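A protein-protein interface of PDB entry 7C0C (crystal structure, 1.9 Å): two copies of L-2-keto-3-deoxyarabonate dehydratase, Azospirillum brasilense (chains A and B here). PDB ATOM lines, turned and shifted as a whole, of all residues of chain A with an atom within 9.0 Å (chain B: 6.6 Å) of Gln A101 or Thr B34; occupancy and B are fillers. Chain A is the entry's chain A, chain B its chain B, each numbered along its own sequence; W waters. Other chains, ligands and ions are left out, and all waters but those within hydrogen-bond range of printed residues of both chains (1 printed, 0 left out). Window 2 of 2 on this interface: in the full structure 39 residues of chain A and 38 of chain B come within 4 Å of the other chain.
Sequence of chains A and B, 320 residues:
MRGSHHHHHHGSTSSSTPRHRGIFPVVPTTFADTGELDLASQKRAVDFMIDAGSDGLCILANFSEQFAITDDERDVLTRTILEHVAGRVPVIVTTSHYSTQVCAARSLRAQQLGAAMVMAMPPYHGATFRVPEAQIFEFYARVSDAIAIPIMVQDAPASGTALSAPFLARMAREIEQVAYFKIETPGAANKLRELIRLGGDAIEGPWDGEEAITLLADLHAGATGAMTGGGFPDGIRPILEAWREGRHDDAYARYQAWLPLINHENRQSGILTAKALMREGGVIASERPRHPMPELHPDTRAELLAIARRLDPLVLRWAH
OG1 of Thr A100 sits at hydrogen-bond distance from ND1 of His B291 (2.6 Å). O of Thr B34 lies close to OE1 of Gln A101, at 3.3 Å. The side-chain amide nitrogen of Gln A101 lies within hydrogen-bond range of the side-chain carboxylate of Glu B36, at 3.3 Å. The side-chain carboxylate (OE1) of Glu A138 is in hydrogen-bond range of a ring nitrogen (NE2) of His B291 (2.9 Å).
A ring nitrogen (ND1) of His A97 lies within hydrogen-bond range of the backbone NH (N) of Ser A99, at 3.1 Å. The backbone NH of Gln A101 lies close to the side-chain hydroxyl of Ser A99 (3.5 Å). The backbone NH of Val A102 is in hydrogen-bond range of the side-chain hydroxyl of Ser A99 (3.1 Å). The guanidinium group (NH1) of Arg A142 is in salt-bridge range of the side-chain carboxylate (OE1) of Glu A138 (3.8 Å). The backbone carbonyl oxygen (O) of Gly B35 is in hydrogen-bond range of the guanidinium group (NE) of Arg B290.
Among the printed residues, merely in contact across the chains: Tyr A98 with Pro B292 (3.0 Å), Ser A99 with His B291 (3.6 Å), Thr A100 with Pro B292 (3.5 Å), Gln A101 with Gly B35 (3.5 Å), Phe A139 with His B291 (3.6 Å) and Arg A142 with His B291 (3.2 Å).
Of chain B, only Thr B34, Gly B35 and Glu B36 come within 4 Å of Gln A101. Printed residues of chain A within 4 Å of Gly B35: Gln A101 (3.5 Å). Of the printed residues of chain A, Glu B36 touches Gln A101 (3.3 Å). Printed residues of chain A within 4 Å of His B291: Ser A99 (3.6 Å), Thr A100 (2.6 Å), Glu A138 (2.9 Å), Phe A139 (3.6 Å) and Arg A142 (3.2 Å). Of the printed residues of chain B, Phe A139 touches His B291. Printed residues of chain B within 4 Å of Ser A99: His B291 (3.6 Å). Ala B32 touches none of the printed residues of chain A. The nearest residue of chain A that does not touch Thr B34 is Arg A142 (7.7 Å).
Hydrophobic or aromatic side chains of chain B within 4 Å of the printed part of chain A: His B291 and Pro B292.
No position is printed for both chains.
Water W1 lies within hydrogen-bond range of the side-chain hydroxyl of Ser A99 (2.7 Å), the backbone carbonyl oxygen of His B291 (2.8 Å), the backbone NH of Gln A101 (3.1 Å) and the backbone NH of Thr A100 (3.2 Å).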
ATOM      1  N   THR A  95      -6.196 -15.017  28.357  1.00  0.00           N
ATOM      2  CA  THR A  95      -5.615 -16.349  28.484  1.00  0.00           C
ATOM      3  C   THR A  95      -5.837 -17.206  27.243  1.00  0.00           C
ATOM      4  O   THR A  95      -5.739 -18.436  27.322  1.00  0.00           O
ATOM      5  CB  THR A  95      -6.191 -17.062  29.709  1.00  0.00           C
ATOM      6  OG1 THR A  95      -7.622 -17.007  29.659  1.00  0.00           O
ATOM      7  CG2 THR A  95      -5.712 -16.405  30.990  1.00  0.00           C
ATOM      8  N   HIS A  97      -5.932 -19.517  24.090  1.00  0.00           N
ATOM      9  CA  HIS A  97      -5.090 -20.567  23.537  1.00  0.00           C
ATOM     10  C   HIS A  97      -6.000 -21.604  22.900  1.00  0.00           C
ATOM     11  O   HIS A  97      -7.128 -21.813  23.355  1.00  0.00           O
ATOM     12  CB  HIS A  97      -4.209 -21.218  24.609  1.00  0.00           C
ATOM     13  CG  HIS A  97      -3.048 -21.979  24.053  1.00  0.00           C
ATOM     14  ND1 HIS A  97      -3.127 -23.313  23.712  1.00  0.00           N
ATOM     15  CD2 HIS A  97      -1.779 -21.594  23.775  1.00  0.00           C
ATOM     16  CE1 HIS A  97      -1.957 -23.717  23.250  1.00  0.00           C
ATOM     17  NE2 HIS A  97      -1.122 -22.693  23.277  1.00  0.00           N
ATOM     18  N   TYR A  98      -5.504 -22.244  21.838  1.00  0.00           N
ATOM     19  CA  TYR A  98      -6.287 -23.289  21.189  1.00  0.00           C
ATOM     20  C   TYR A  98      -6.634 -24.395  22.176  1.00  0.00           C
ATOM     21  O   TYR A  98      -7.798 -24.792  22.296  1.00  0.00           O
ATOM     22  CB  TYR A  98      -5.532 -23.860  19.989  1.00  0.00           C
ATOM     23  CG  TYR A  98      -6.325 -24.870  19.187  1.00  0.00           C
ATOM     24  CD1 TYR A  98      -6.331 -26.221  19.531  1.00  0.00           C
ATOM     25  CD2 TYR A  98      -7.071 -24.476  18.083  1.00  0.00           C
ATOM     26  CE1 TYR A  98      -7.060 -27.145  18.798  1.00  0.00           C
ATOM     27  CE2 TYR A  98      -7.800 -25.392  17.345  1.00  0.00           C
ATOM     28  CZ  TYR A  98      -7.790 -26.723  17.705  1.00  0.00           C
ATOM     29  OH  TYR A  98      -8.514 -27.631  16.967  1.00  0.00           O
ATOM     30  N   SER A  99      -5.634 -24.888  22.905  1.00  0.00           N
ATOM     31  CA  SER A  99      -5.838 -26.024  23.790  1.00  0.00           C
ATOM     32  C   SER A  99      -6.666 -25.628  25.005  1.00  0.00           C
ATOM     33  O   SER A  99      -6.376 -24.632  25.675  1.00  0.00           O
ATOM     34  CB  SER A  99      -4.498 -26.595  24.240  1.00  0.00           C
ATOM     35  OG  SER A  99      -4.646 -27.298  25.461  1.00  0.00           O
ATOM     36  N   THR A 100      -7.692 -26.431  25.293  1.00  0.00           N
ATOM     37  CA  THR A 100      -8.572 -26.162  26.427  1.00  0.00           C
ATOM     38  C   THR A 100      -7.805 -26.210  27.743  1.00  0.00           C
ATOM     39  O   THR A 100      -7.900 -25.289  28.563  1.00  0.00           O
ATOM     40  CB  THR A 100      -9.719 -27.172  26.442  1.00  0.00           C
ATOM     41  OG1 THR A 100     -10.512 -27.012  25.258  1.00  0.00           O
ATOM     42  CG2 THR A 100     -10.596 -26.972  27.668  1.00  0.00           C
ATOM     43  N   GLN A 101      -7.040 -27.284  27.964  1.00  0.00           N
ATOM     44  CA  GLN A 101      -6.302 -27.413  29.214  1.00  0.00           C
ATOM     45  C   GLN A 101      -5.272 -26.298  29.365  1.00  0.00           C
ATOM     46  O   GLN A 101      -5.046 -25.802  30.475  1.00  0.00           O
ATOM     47  CB  GLN A 101      -5.634 -28.787  29.295  1.00  0.00           C
ATOM     48  CG  GLN A 101      -6.531 -29.935  28.859  1.00  0.00           C
ATOM     49  CD  GLN A 101      -5.745 -31.147  28.407  1.00  0.00           C
ATOM     50  OE1 GLN A 101      -6.233 -31.960  27.621  1.00  0.00           O
ATOM     51  NE2 GLN A 101      -4.524 -31.278  28.907  1.00  0.00           N
ATOM     52  N   VAL A 102      -4.651 -25.876  28.260  1.00  0.00           N
ATOM     53  CA  VAL A 102      -3.691 -24.779  28.331  1.00  0.00           C
ATOM     54  C   VAL A 102      -4.391 -23.483  28.721  1.00  0.00           C
ATOM     55  O   VAL A 102      -3.881 -22.706  29.537  1.00  0.00           O
ATOM     56  CB  VAL A 102      -2.935 -24.640  26.997  1.00  0.00           C
ATOM     57  CG1 VAL A 102      -2.092 -23.374  26.995  1.00  0.00           C
ATOM     58  CG2 VAL A 102      -2.064 -25.859  26.762  1.00  0.00           C
ATOM     59  N   CYS A 103      -5.574 -23.234  28.155  1.00  0.00           N
ATOM     60  CA  CYS A 103      -6.328 -22.047  28.544  1.00  0.00           C
ATOM     61  C   CYS A 103      -6.816 -22.156  29.981  1.00  0.00           C
ATOM     62  O   CYS A 103      -6.806 -21.166  30.722  1.00  0.00           O
ATOM     63  CB  CYS A 103      -7.504 -21.823  27.594  1.00  0.00           C
ATOM     64  SG  CYS A 103      -8.417 -20.282  27.921  1.00  0.00           S
ATOM     65  N   ALA A 104      -7.244 -23.351  30.396  1.00  0.00           N
ATOM     66  CA  ALA A 104      -7.680 -23.536  31.776  1.00  0.00           C
ATOM     67  C   ALA A 104      -6.532 -23.307  32.751  1.00  0.00           C
ATOM     68  O   ALA A 104      -6.704 -22.643  33.780  1.00  0.00           O
ATOM     69  CB  ALA A 104      -8.271 -24.932  31.959  1.00  0.00           C
ATOM     70  N   ALA A 105      -5.346 -23.837  32.433  1.00  0.00           N
ATOM     71  CA  ALA A 105      -4.199 -23.688  33.324  1.00  0.00           C
ATOM     72  C   ALA A 105      -3.725 -22.241  33.384  1.00  0.00           C
ATOM     73  O   ALA A 105      -3.296 -21.766  34.442  1.00  0.00           O
ATOM     74  CB  ALA A 105      -3.064 -24.607  32.875  1.00  0.00           C
ATOM     75  N   ARG A 106      -3.789 -21.526  32.258  1.00  0.00           N
ATOM     76  CA  ARG A 106      -3.452 -20.106  32.269  1.00  0.00           C
ATOM     77  C   ARG A 106      -4.466 -19.311  33.081  1.00  0.00           C
ATOM     78  O   ARG A 106      -4.098 -18.386  33.815  1.00  0.00           O
ATOM     79  CB  ARG A 106      -3.378 -19.570  30.839  1.00  0.00           C
ATOM     80  CG  ARG A 106      -2.095 -19.924  30.097  1.00  0.00           C
ATOM     81  CD  ARG A 106      -2.009 -19.181  28.771  1.00  0.00           C
ATOM     82  NE  ARG A 106      -0.858 -19.594  27.972  1.00  0.00           N
ATOM     83  CZ  ARG A 106      -0.646 -19.212  26.716  1.00  0.00           C
ATOM     84  NH1 ARG A 106       0.425 -19.636  26.059  1.00  0.00           N
ATOM     85  NH2 ARG A 106      -1.510 -18.404  26.113  1.00  0.00           N
ATOM     86  N   SER A 107      -5.748 -19.659  32.961  1.00  0.00           N
ATOM     87  CA  SER A 107      -6.785 -18.934  33.689  1.00  0.00           C
ATOM     88  C   SER A 107      -6.707 -19.215  35.183  1.00  0.00           C
ATOM     89  O   SER A 107      -6.984 -18.329  36.001  1.00  0.00           O
ATOM     90  CB  SER A 107      -8.164 -19.305  33.144  1.00  0.00           C
ATOM     91  OG  SER A 107      -8.220 -19.116  31.740  1.00  0.00           O
ATOM     92  N   LEU A 108      -6.339 -20.441  35.558  1.00  0.00           N
ATOM     93  CA  LEU A 108      -6.168 -20.760  36.972  1.00  0.00           C
ATOM     94  C   LEU A 108      -4.973 -20.016  37.554  1.00  0.00           C
ATOM     95  O   LEU A 108      -5.068 -19.413  38.631  1.00  0.00           O
ATOM     96  CB  LEU A 108      -6.005 -22.268  37.151  1.00  0.00           C
ATOM     97  CG  LEU A 108      -5.933 -22.758  38.599  1.00  0.00           C
ATOM     98  CD1 LEU A 108      -7.269 -22.550  39.297  1.00  0.00           C
ATOM     99  CD2 LEU A 108      -5.509 -24.221  38.664  1.00  0.00           C
ATOM    100  N   ARG A 109      -3.839 -20.043  36.850  1.00  0.00           N
ATOM    101  CA  ARG A 109      -2.659 -19.316  37.304  1.00  0.00           C
ATOM    102  C   ARG A 109      -2.947 -17.824  37.428  1.00  0.00           C
ATOM    103  O   ARG A 109      -2.535 -17.183  38.403  1.00  0.00           O
ATOM    104  CB  ARG A 109      -1.496 -19.569  36.345  1.00  0.00           C
ATOM    105  CG  ARG A 109      -0.438 -18.481  36.334  1.00  0.00           C
ATOM    106  CD  ARG A 109       0.432 -18.546  37.576  1.00  0.00           C
ATOM    107  NE  ARG A 109       1.816 -18.177  37.292  1.00  0.00           N
ATOM    108  CZ  ARG A 109       2.785 -18.164  38.200  1.00  0.00           C
ATOM    109  NH1 ARG A 109       4.016 -17.813  37.858  1.00  0.00           N
ATOM    110  NH2 ARG A 109       2.518 -18.489  39.457  1.00  0.00           N
ATOM    111  N   GLU A 138     -17.753 -26.729  24.920  1.00  0.00           N
ATOM    112  CA  GLU A 138     -16.991 -27.527  25.873  1.00  0.00           C
ATOM    113  C   GLU A 138     -15.717 -26.807  26.294  1.00  0.00           C
ATOM    114  O   GLU A 138     -15.285 -26.921  27.447  1.00  0.00           O
ATOM    115  CB  GLU A 138     -16.658 -28.889  25.269  1.00  0.00           C
ATOM    116  CG  GLU A 138     -17.869 -29.687  24.820  1.00  0.00           C
ATOM    117  CD  GLU A 138     -17.491 -31.004  24.167  1.00  0.00           C
ATOM    118  OE1 GLU A 138     -16.355 -31.120  23.658  1.00  0.00           O
ATOM    119  OE2 GLU A 138     -18.334 -31.926  24.165  1.00  0.00           O
ATOM    120  N   PHE A 139     -15.102 -26.069  25.367  1.00  0.00           N
ATOM    121  CA  PHE A 139     -13.897 -25.311  25.683  1.00  0.00           C
ATOM    122  C   PHE A 139     -14.160 -24.320  26.809  1.00  0.00           C
ATOM    123  O   PHE A 139     -13.421 -24.277  27.799  1.00  0.00           O
ATOM    124  CB  PHE A 139     -13.394 -24.598  24.423  1.00  0.00           C
ATOM    125  CG  PHE A 139     -12.270 -23.632  24.667  1.00  0.00           C
ATOM    126  CD1 PHE A 139     -12.530 -22.298  24.947  1.00  0.00           C
ATOM    127  CD2 PHE A 139     -10.952 -24.051  24.594  1.00  0.00           C
ATOM    128  CE1 PHE A 139     -11.496 -21.408  25.166  1.00  0.00           C
ATOM    129  CE2 PHE A 139      -9.915 -23.162  24.809  1.00  0.00           C
ATOM    130  CZ  PHE A 139     -10.190 -21.840  25.097  1.00  0.00           C
ATOM    131  N   ARG A 142     -15.195 -26.062  30.205  1.00  0.00           N
ATOM    132  CA  ARG A 142     -14.117 -26.690  30.961  1.00  0.00           C
ATOM    133  C   ARG A 142     -13.229 -25.660  31.646  1.00  0.00           C
ATOM    134  O   ARG A 142     -12.773 -25.883  32.774  1.00  0.00           O
ATOM    135  CB  ARG A 142     -13.294 -27.593  30.045  1.00  0.00           C
ATOM    136  CG  ARG A 142     -14.027 -28.867  29.668  1.00  0.00           C
ATOM    137  CD  ARG A 142     -13.305 -29.651  28.593  1.00  0.00           C
ATOM    138  NE  ARG A 142     -14.200 -30.628  27.984  1.00  0.00           N
ATOM    139  CZ  ARG A 142     -13.799 -31.712  27.329  1.00  0.00           C
ATOM    140  NH1 ARG A 142     -14.698 -32.540  26.813  1.00  0.00           N
ATOM    141  NH2 ARG A 142     -12.505 -31.973  27.199  1.00  0.00           N
ATOM    142  N   VAL A 143     -12.966 -24.530  30.983  1.00  0.00           N
ATOM    143  CA  VAL A 143     -12.231 -23.453  31.636  1.00  0.00           C
ATOM    144  C   VAL A 143     -13.026 -22.917  32.817  1.00  0.00           C
ATOM    145  O   VAL A 143     -12.450 -22.505  33.831  1.00  0.00           O
ATOM    146  CB  VAL A 143     -11.894 -22.349  30.612  1.00  0.00           C
ATOM    147  CG1 VAL A 143     -11.285 -21.137  31.297  1.00  0.00           C
ATOM    148  CG2 VAL A 143     -10.944 -22.893  29.552  1.00  0.00           C
ATOM    149  N   ALA A 146     -12.677 -25.095  35.992  1.00  0.00           N
ATOM    150  CA  ALA A 146     -11.372 -25.040  36.637  1.00  0.00           C
ATOM    151  C   ALA A 146     -11.148 -23.789  37.473  1.00  0.00           C
ATOM    152  O   ALA A 146     -10.246 -23.786  38.317  1.00  0.00           O
ATOM    153  CB  ALA A 146     -10.260 -25.135  35.587  1.00  0.00           C
ATOM    154  N   ILE A 147     -11.926 -22.726  37.265  1.00  0.00           N
ATOM    155  CA  ILE A 147     -11.664 -21.445  37.909  1.00  0.00           C
ATOM    156  C   ILE A 147     -12.905 -20.983  38.664  1.00  0.00           C
ATOM    157  O   ILE A 147     -14.007 -21.506  38.488  1.00  0.00           O
ATOM    158  CB  ILE A 147     -11.212 -20.367  36.903  1.00  0.00           C
ATOM    159  CG1 ILE A 147     -12.399 -19.864  36.080  1.00  0.00           C
ATOM    160  CG2 ILE A 147     -10.123 -20.911  35.992  1.00  0.00           C
ATOM    161  CD1 ILE A 147     -12.013 -18.839  35.034  1.00  0.00           C
ATOM    162  N   PHE B  31      -0.475 -37.685  22.690  1.00  0.00           N
ATOM    163  CA  PHE B  31      -0.963 -37.384  24.025  1.00  0.00           C
ATOM    164  C   PHE B  31      -1.475 -38.655  24.689  1.00  0.00           C
ATOM    165  O   PHE B  31      -1.832 -39.631  24.027  1.00  0.00           O
ATOM    166  CB  PHE B  31      -2.091 -36.347  23.986  1.00  0.00           C
ATOM    167  CG  PHE B  31      -1.770 -35.123  23.183  1.00  0.00           C
ATOM    168  CD1 PHE B  31      -0.810 -34.226  23.615  1.00  0.00           C
ATOM    169  CD2 PHE B  31      -2.441 -34.863  21.999  1.00  0.00           C
ATOM    170  CE1 PHE B  31      -0.519 -33.092  22.878  1.00  0.00           C
ATOM    171  CE2 PHE B  31      -2.154 -33.734  21.258  1.00  0.00           C
ATOM    172  CZ  PHE B  31      -1.192 -32.848  21.696  1.00  0.00           C
ATOM    173  N   ALA B  32      -1.510 -38.629  26.017  1.00  0.00           N
ATOM    174  CA  ALA B  32      -2.305 -39.602  26.745  1.00  0.00           C
ATOM    175  C   ALA B  32      -3.784 -39.268  26.565  1.00  0.00           C
ATOM    176  O   ALA B  32      -4.154 -38.299  25.893  1.00  0.00           O
ATOM    177  CB  ALA B  32      -1.906 -39.623  28.218  1.00  0.00           C
ATOM    178  N   ASP B  33      -4.650 -40.080  27.172  1.00  0.00           N
ATOM    179  CA  ASP B  33      -6.083 -39.838  27.038  1.00  0.00           C
ATOM    180  C   ASP B  33      -6.476 -38.497  27.646  1.00  0.00           C
ATOM    181  O   ASP B  33      -7.337 -37.791  27.108  1.00  0.00           O
ATOM    182  CB  ASP B  33      -6.874 -40.975  27.684  1.00  0.00           C
ATOM    183  CG  ASP B  33      -7.006 -42.180  26.774  1.00  0.00           C
ATOM    184  OD1 ASP B  33      -5.965 -42.748  26.383  1.00  0.00           O
ATOM    185  OD2 ASP B  33      -8.151 -42.556  26.447  1.00  0.00           O
ATOM    186  N   THR B  34      -5.842 -38.121  28.752  1.00  0.00           N
ATOM    187  CA  THR B  34      -6.178 -36.893  29.461  1.00  0.00           C
ATOM    188  C   THR B  34      -5.432 -35.668  28.941  1.00  0.00           C
ATOM    189  O   THR B  34      -5.593 -34.582  29.506  1.00  0.00           O
ATOM    190  CB  THR B  34      -5.912 -37.067  30.959  1.00  0.00           C
ATOM    191  OG1 THR B  34      -4.524 -37.348  31.172  1.00  0.00           O
ATOM    192  CG2 THR B  34      -6.751 -38.210  31.512  1.00  0.00           C
ATOM    193  N   GLY B  35      -4.621 -35.810  27.892  1.00  0.00           N
ATOM    194  CA  GLY B  35      -4.102 -34.670  27.164  1.00  0.00           C
ATOM    195  C   GLY B  35      -2.654 -34.315  27.429  1.00  0.00           C
ATOM    196  O   GLY B  35      -2.103 -33.476  26.705  1.00  0.00           O
ATOM    197  N   GLU B  36      -2.022 -34.908  28.435  1.00  0.00           N
ATOM    198  CA  GLU B  36      -0.619 -34.606  28.671  1.00  0.00           C
ATOM    199  C   GLU B  36       0.255 -35.366  27.678  1.00  0.00           C
ATOM    200  O   GLU B  36      -0.163 -36.360  27.077  1.00  0.00           O
ATOM    201  CB  GLU B  36      -0.223 -34.949  30.108  1.00  0.00           C
ATOM    202  CG  GLU B  36      -1.361 -34.844  31.122  1.00  0.00           C
ATOM    203  CD  GLU B  36      -2.051 -33.489  31.111  1.00  0.00           C
ATOM    204  OE1 GLU B  36      -3.301 -33.459  31.077  1.00  0.00           O
ATOM    205  OE2 GLU B  36      -1.345 -32.457  31.138  1.00  0.00           O
ATOM    206  N   SER B 286      -2.414 -43.770  22.711  1.00  0.00           N
ATOM    207  CA  SER B 286      -3.655 -43.028  22.537  1.00  0.00           C
ATOM    208  C   SER B 286      -3.616 -42.235  21.239  1.00  0.00           C
ATOM    209  O   SER B 286      -2.597 -41.629  20.897  1.00  0.00           O
ATOM    210  CB  SER B 286      -3.907 -42.081  23.719  1.00  0.00           C
ATOM    211  OG  SER B 286      -5.155 -41.420  23.592  1.00  0.00           O
ATOM    212  N   PRO B 289      -6.832 -36.455  19.986  1.00  0.00           N
ATOM    213  CA  PRO B 289      -6.283 -35.101  19.894  1.00  0.00           C
ATOM    214  C   PRO B 289      -6.455 -34.379  21.217  1.00  0.00           C
ATOM    215  O   PRO B 289      -7.195 -34.809  22.104  1.00  0.00           O
ATOM    216  CB  PRO B 289      -7.124 -34.457  18.792  1.00  0.00           C
ATOM    217  CG  PRO B 289      -8.452 -35.135  18.922  1.00  0.00           C
ATOM    218  CD  PRO B 289      -8.148 -36.562  19.329  1.00  0.00           C
ATOM    219  N   ARG B 290      -5.752 -33.264  21.352  1.00  0.00           N
ATOM    220  CA  ARG B 290      -6.003 -32.398  22.492  1.00  0.00           C
ATOM    221  C   ARG B 290      -7.302 -31.639  22.262  1.00  0.00           C
ATOM    222  O   ARG B 290      -7.533 -31.099  21.176  1.00  0.00           O
ATOM    223  CB  ARG B 290      -4.838 -31.436  22.713  1.00  0.00           C
ATOM    224  CG  ARG B 290      -4.108 -31.679  24.022  1.00  0.00           C
ATOM    225  CD  ARG B 290      -2.926 -30.747  24.199  1.00  0.00           C
ATOM    226  NE  ARG B 290      -1.943 -31.303  25.124  1.00  0.00           N
ATOM    227  CZ  ARG B 290      -0.850 -30.662  25.525  1.00  0.00           C
ATOM    228  NH1 ARG B 290      -0.604 -29.436  25.083  1.00  0.00           N
ATOM    229  NH2 ARG B 290      -0.007 -31.242  26.370  1.00  0.00           N
ATOM    230  N   HIS B 291      -8.169 -31.646  23.269  1.00  0.00           N
ATOM    231  CA  HIS B 291      -9.392 -30.862  23.204  1.00  0.00           C
ATOM    232  C   HIS B 291      -9.035 -29.402  22.939  1.00  0.00           C
ATOM    233  O   HIS B 291      -8.012 -28.915  23.438  1.00  0.00           O
ATOM    234  CB  HIS B 291     -10.169 -31.001  24.516  1.00  0.00           C
ATOM    235  CG  HIS B 291     -11.567 -30.470  24.455  1.00  0.00           C
ATOM    236  ND1 HIS B 291     -11.878 -29.162  24.756  1.00  0.00           N
ATOM    237  CD2 HIS B 291     -12.735 -31.066  24.116  1.00  0.00           C
ATOM    238  CE1 HIS B 291     -13.178 -28.976  24.611  1.00  0.00           C
ATOM    239  NE2 HIS B 291     -13.721 -30.116  24.223  1.00  0.00           N
ATOM    240  N   PRO B 292      -9.849 -28.663  22.165  1.00  0.00           N
ATOM    241  CA  PRO B 292     -11.159 -28.985  21.595  1.00  0.00           C
ATOM    242  C   PRO B 292     -11.172 -29.458  20.146  1.00  0.00           C
ATOM    243  O   PRO B 292     -12.227 -29.367  19.519  1.00  0.00           O
ATOM    244  CB  PRO B 292     -11.888 -27.649  21.702  1.00  0.00           C
ATOM    245  CG  PRO B 292     -10.809 -26.658  21.412  1.00  0.00           C
ATOM    246  CD  PRO B 292      -9.511 -27.251  21.923  1.00  0.00           C
HETATM  247  O   HOH W   1      -6.468 -29.327  25.702  1.00  0.00           O
